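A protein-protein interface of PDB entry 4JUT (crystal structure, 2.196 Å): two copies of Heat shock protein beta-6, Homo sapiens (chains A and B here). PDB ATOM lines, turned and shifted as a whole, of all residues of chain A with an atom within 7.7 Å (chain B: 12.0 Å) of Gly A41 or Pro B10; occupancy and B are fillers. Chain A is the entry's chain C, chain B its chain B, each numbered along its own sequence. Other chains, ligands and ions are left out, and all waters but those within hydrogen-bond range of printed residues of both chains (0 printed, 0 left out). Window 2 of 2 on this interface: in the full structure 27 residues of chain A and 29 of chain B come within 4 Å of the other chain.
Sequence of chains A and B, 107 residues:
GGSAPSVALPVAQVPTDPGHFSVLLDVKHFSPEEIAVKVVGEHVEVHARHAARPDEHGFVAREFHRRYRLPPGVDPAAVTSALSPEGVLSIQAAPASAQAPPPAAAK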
ATOM      1  N   LYS A  38     -18.581  -8.726  -8.321  1.00  0.00           N
ATOM      2  CA  LYS A  38     -17.994  -7.496  -7.802  1.00  0.00           C
ATOM      3  C   LYS A  38     -17.109  -6.742  -8.785  1.00  0.00           C
ATOM      4  O   LYS A  38     -16.650  -7.296  -9.780  1.00  0.00           O
ATOM      5  CB  LYS A  38     -17.269  -7.731  -6.470  1.00  0.00           C
ATOM      6  CG  LYS A  38     -16.310  -8.883  -6.439  1.00  0.00           C
ATOM      7  CD  LYS A  38     -16.192  -9.375  -5.007  1.00  0.00           C
ATOM      8  CE  LYS A  38     -15.012 -10.312  -4.816  1.00  0.00           C
ATOM      9  NZ  LYS A  38     -15.189 -11.147  -3.597  1.00  0.00           N
ATOM     10  N   VAL A  39     -16.913  -5.454  -8.515  1.00  0.00           N
ATOM     11  CA  VAL A  39     -15.986  -4.662  -9.294  1.00  0.00           C
ATOM     12  C   VAL A  39     -14.751  -4.437  -8.444  1.00  0.00           C
ATOM     13  O   VAL A  39     -14.831  -3.937  -7.319  1.00  0.00           O
ATOM     14  CB  VAL A  39     -16.596  -3.329  -9.719  1.00  0.00           C
ATOM     15  CG1 VAL A  39     -15.540  -2.480 -10.379  1.00  0.00           C
ATOM     16  CG2 VAL A  39     -17.734  -3.567 -10.679  1.00  0.00           C
ATOM     17  N   VAL A  40     -13.611  -4.862  -8.961  1.00  0.00           N
ATOM     18  CA  VAL A  40     -12.363  -4.741  -8.222  1.00  0.00           C
ATOM     19  C   VAL A  40     -11.350  -4.034  -9.096  1.00  0.00           C
ATOM     20  O   VAL A  40     -10.886  -4.592 -10.094  1.00  0.00           O
ATOM     21  CB  VAL A  40     -11.817  -6.106  -7.808  1.00  0.00           C
ATOM     22  CG1 VAL A  40     -10.450  -5.946  -7.164  1.00  0.00           C
ATOM     23  CG2 VAL A  40     -12.783  -6.774  -6.845  1.00  0.00           C
ATOM     24  N   GLY A  41     -11.029  -2.797  -8.731  1.00  0.00           N
ATOM     25  CA  GLY A  41     -10.184  -1.957  -9.564  1.00  0.00           C
ATOM     26  C   GLY A  41     -10.835  -1.732 -10.913  1.00  0.00           C
ATOM     27  O   GLY A  41     -11.955  -1.219 -10.992  1.00  0.00           O
ATOM     28  N   GLU A  42     -10.150  -2.144 -11.973  1.00  0.00           N
ATOM     29  CA  GLU A  42     -10.674  -1.985 -13.329  1.00  0.00           C
ATOM     30  C   GLU A  42     -11.348  -3.249 -13.866  1.00  0.00           C
ATOM     31  O   GLU A  42     -11.664  -3.336 -15.047  1.00  0.00           O
ATOM     32  CB  GLU A  42      -9.556  -1.543 -14.282  1.00  0.00           C
ATOM     33  CG  GLU A  42      -8.282  -2.376 -14.174  1.00  0.00           C
ATOM     34  CD  GLU A  42      -7.161  -1.872 -15.074  1.00  0.00           C
ATOM     35  OE1 GLU A  42      -7.460  -1.395 -16.193  1.00  0.00           O
ATOM     36  OE2 GLU A  42      -5.982  -1.950 -14.658  1.00  0.00           O
ATOM     37  N   HIS A  43     -11.576  -4.226 -13.000  1.00  0.00           N
ATOM     38  CA  HIS A  43     -12.111  -5.499 -13.454  1.00  0.00           C
ATOM     39  C   HIS A  43     -13.460  -5.875 -12.827  1.00  0.00           C
ATOM     40  O   HIS A  43     -13.717  -5.591 -11.655  1.00  0.00           O
ATOM     41  CB  HIS A  43     -11.094  -6.594 -13.169  1.00  0.00           C
ATOM     42  CG  HIS A  43      -9.834  -6.467 -13.963  1.00  0.00           C
ATOM     43  ND1 HIS A  43      -8.794  -5.649 -13.578  1.00  0.00           N
ATOM     44  CD2 HIS A  43      -9.440  -7.063 -15.114  1.00  0.00           C
ATOM     45  CE1 HIS A  43      -7.815  -5.745 -14.460  1.00  0.00           C
ATOM     46  NE2 HIS A  43      -8.182  -6.597 -15.401  1.00  0.00           N
ATOM     47  N   VAL A  44     -14.318  -6.518 -13.610  1.00  0.00           N
ATOM     48  CA  VAL A  44     -15.512  -7.145 -13.057  1.00  0.00           C
ATOM     49  C   VAL A  44     -15.174  -8.596 -12.761  1.00  0.00           C
ATOM     50  O   VAL A  44     -14.646  -9.304 -13.614  1.00  0.00           O
ATOM     51  CB  VAL A  44     -16.696  -7.130 -14.032  1.00  0.00           C
ATOM     52  CG1 VAL A  44     -17.873  -7.895 -13.436  1.00  0.00           C
ATOM     53  CG2 VAL A  44     -17.112  -5.720 -14.339  1.00  0.00           C
ATOM     54  N   GLU A  45     -15.469  -9.044 -11.552  1.00  0.00           N
ATOM     55  CA  GLU A  45     -15.236 -10.442 -11.219  1.00  0.00           C
ATOM     56  C   GLU A  45     -16.565 -11.100 -10.949  1.00  0.00           C
ATOM     57  O   GLU A  45     -17.507 -10.473 -10.441  1.00  0.00           O
ATOM     58  CB  GLU A  45     -14.309 -10.589 -10.007  1.00  0.00           C
ATOM     59  CG  GLU A  45     -12.923  -9.982 -10.210  1.00  0.00           C
ATOM     60  CD  GLU A  45     -11.987 -10.254  -9.041  1.00  0.00           C
ATOM     61  OE1 GLU A  45     -12.453 -10.838  -8.036  1.00  0.00           O
ATOM     62  OE2 GLU A  45     -10.790  -9.886  -9.126  1.00  0.00           O
ATOM     63  N   LEU A  70     -12.932  -3.889 -17.421  1.00  0.00           N
ATOM     64  CA  LEU A  70     -13.874  -2.858 -17.846  1.00  0.00           C
ATOM     65  C   LEU A  70     -13.262  -2.052 -18.990  1.00  0.00           C
ATOM     66  O   LEU A  70     -12.049  -1.819 -18.991  1.00  0.00           O
ATOM     67  CB  LEU A  70     -14.233  -1.927 -16.685  1.00  0.00           C
ATOM     68  CG  LEU A  70     -15.288  -2.447 -15.721  1.00  0.00           C
ATOM     69  CD1 LEU A  70     -15.687  -1.345 -14.773  1.00  0.00           C
ATOM     70  CD2 LEU A  70     -16.492  -2.971 -16.520  1.00  0.00           C
ATOM     71  N   VAL A  74     -15.232   3.757 -18.383  1.00  0.00           N
ATOM     72  CA  VAL A  74     -16.444   3.259 -17.738  1.00  0.00           C
ATOM     73  C   VAL A  74     -16.361   3.379 -16.213  1.00  0.00           C
ATOM     74  O   VAL A  74     -15.341   3.057 -15.610  1.00  0.00           O
ATOM     75  CB  VAL A  74     -16.720   1.798 -18.153  1.00  0.00           C
ATOM     76  CG1 VAL A  74     -17.926   1.242 -17.422  1.00  0.00           C
ATOM     77  CG2 VAL A  74     -16.918   1.712 -19.658  1.00  0.00           C
ATOM     78  N   ASP A  75     -17.437   3.857 -15.599  1.00  0.00           N
ATOM     79  CA  ASP A  75     -17.515   3.991 -14.146  1.00  0.00           C
ATOM     80  C   ASP A  75     -18.021   2.705 -13.487  1.00  0.00           C
ATOM     81  O   ASP A  75     -19.146   2.276 -13.745  1.00  0.00           O
ATOM     82  CB  ASP A  75     -18.446   5.157 -13.793  1.00  0.00           C
ATOM     83  CG  ASP A  75     -18.523   5.419 -12.298  1.00  0.00           C
ATOM     84  OD1 ASP A  75     -17.619   4.967 -11.562  1.00  0.00           O
ATOM     85  OD2 ASP A  75     -19.490   6.089 -11.862  1.00  0.00           O
ATOM     86  N   PRO A  76     -17.184   2.086 -12.637  1.00  0.00           N
ATOM     87  CA  PRO A  76     -17.512   0.919 -11.808  1.00  0.00           C
ATOM     88  C   PRO A  76     -18.883   0.996 -11.136  1.00  0.00           C
ATOM     89  O   PRO A  76     -19.579  -0.017 -11.024  1.00  0.00           O
ATOM     90  CB  PRO A  76     -16.415   0.948 -10.747  1.00  0.00           C
ATOM     91  CG  PRO A  76     -15.230   1.446 -11.500  1.00  0.00           C
ATOM     92  CD  PRO A  76     -15.759   2.440 -12.519  1.00  0.00           C
ATOM     93  N   PRO B  10     -10.003  -0.435  -4.616  1.00  0.00           N
ATOM     94  CA  PRO B  10     -11.354   0.098  -4.834  1.00  0.00           C
ATOM     95  C   PRO B  10     -12.335  -1.048  -5.059  1.00  0.00           C
ATOM     96  O   PRO B  10     -12.360  -1.617  -6.154  1.00  0.00           O
ATOM     97  CB  PRO B  10     -11.210   0.925  -6.123  1.00  0.00           C
ATOM     98  CG  PRO B  10      -9.755   1.190  -6.259  1.00  0.00           C
ATOM     99  CD  PRO B  10      -9.068  -0.011  -5.668  1.00  0.00           C
ATOM    100  N   VAL B  11     -13.121  -1.386  -4.037  1.00  0.00           N
ATOM    101  CA  VAL B  11     -13.986  -2.564  -4.099  1.00  0.00           C
ATOM    102  C   VAL B  11     -15.467  -2.262  -3.930  1.00  0.00           C
ATOM    103  O   VAL B  11     -15.890  -1.691  -2.922  1.00  0.00           O
ATOM    104  CB  VAL B  11     -13.592  -3.613  -3.055  1.00  0.00           C
ATOM    105  CG1 VAL B  11     -14.455  -4.861  -3.217  1.00  0.00           C
ATOM    106  CG2 VAL B  11     -12.126  -3.954  -3.200  1.00  0.00           C
ATOM    107  N   ALA B  12     -16.244  -2.672  -4.928  1.00  0.00           N
ATOM    108  CA  ALA B  12     -17.688  -2.501  -4.917  1.00  0.00           C
ATOM    109  C   ALA B  12     -18.403  -3.839  -5.144  1.00  0.00           C
ATOM    110  O   ALA B  12     -17.952  -4.676  -5.928  1.00  0.00           O
ATOM    111  CB  ALA B  12     -18.095  -1.508  -5.986  1.00  0.00           C
ATOM    112  N   GLN B  13     -19.521  -4.040  -4.463  1.00  0.00           N
ATOM    113  CA  GLN B  13     -20.371  -5.177  -4.773  1.00  0.00           C
ATOM    114  C   GLN B  13     -21.430  -4.750  -5.791  1.00  0.00           C
ATOM    115  O   GLN B  13     -21.999  -3.653  -5.696  1.00  0.00           O
ATOM    116  CB  GLN B  13     -21.014  -5.747  -3.510  1.00  0.00           C
ATOM    117  CG  GLN B  13     -20.026  -5.947  -2.368  1.00  0.00           C
ATOM    118  CD  GLN B  13     -20.462  -7.028  -1.383  1.00  0.00           C
ATOM    119  OE1 GLN B  13     -21.532  -6.944  -0.776  1.00  0.00           O
ATOM    120  NE2 GLN B  13     -19.626  -8.054  -1.223  1.00  0.00           N
ATOM    121  N   VAL B  14     -21.656  -5.603  -6.786  1.00  0.00           N
ATOM    122  CA  VAL B  14     -22.687  -5.372  -7.790  1.00  0.00           C
ATOM    123  C   VAL B  14     -23.895  -6.238  -7.435  1.00  0.00           C
ATOM    124  O   VAL B  14     -23.823  -7.468  -7.491  1.00  0.00           O
ATOM    125  CB  VAL B  14     -22.190  -5.789  -9.192  1.00  0.00           C
ATOM    126  CG1 VAL B  14     -23.252  -5.514 -10.269  1.00  0.00           C
ATOM    127  CG2 VAL B  14     -20.870  -5.133  -9.513  1.00  0.00           C
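Lys A38 touches Ala B12. Pro B10 touches Val A39. Val A39 touches Val B11 (O to CA, 3.6 Å). CG2 of Val A39 touches CG2 of Val B14, 3.7 Å away. Val A40 touches Pro B10.
O of Lys A38 is in hydrogen-bond range of N of Glu A45 (2.8 Å).
Printed residues of chain B within 4 Å of Lys A38: Ala B12. Val A39 touches four residues of chain B. Val A40 touches just one residue of chain B: Pro B10 (3.7 Å). Gly A41 touches just one residue of chain B: Pro B10. No residue of chain B comes within 4 Å of Glu A42. His A43 touches none of the printed residues of chain B. Glu A45 touches none of the printed residues of chain B. No residue of chain B comes within 4 Å of Pro A76. Of chain A, only Val A39 (3.6 Å), Val A40 (3.7 Å) and Gly A41 (3.1 Å) come within 4 Å of Pro B10. Printed residues of chain A within 4 Å of Val B11: Val A39. Gln B13 touches none of the printed residues of chain A. Of the printed residues of chain A, Val B14 touches Val A39 (3.7 Å). The nearest residue of chain B that does not touch Gly A41 is Val B11 (5.3 Å). The nearest printed residue of chain A that does not touch Val B14 is Lys A38 (4.1 Å).
No position is printed for both chains.
The backbone NH (N) of Gly A41 lies within hydrogen-bond range of the backbone carbonyl oxygen (O) of Pro B10 (3.1 Å). N of Val A39 is in hydrogen-bond range of O of Ala B12, at 2.9 Å.
Printed residues of chain A that touch a printed residue of chain B: Lys A38, Val A39, Val A40 and Gly A41. Hydrophobic or aromatic side chains of chain A within 4 Å of the printed part of chain B: Val A39. Hydrophobic or aromatic side chains of chain B that line the printed part of chain A: Val B14. Among the printed residues, 7 pairs touch across the chains. Among the printed residues, no Asp or Glu carboxylate lies within 4 Å of a Lys or Arg side-chain nitrogen of the other chain.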
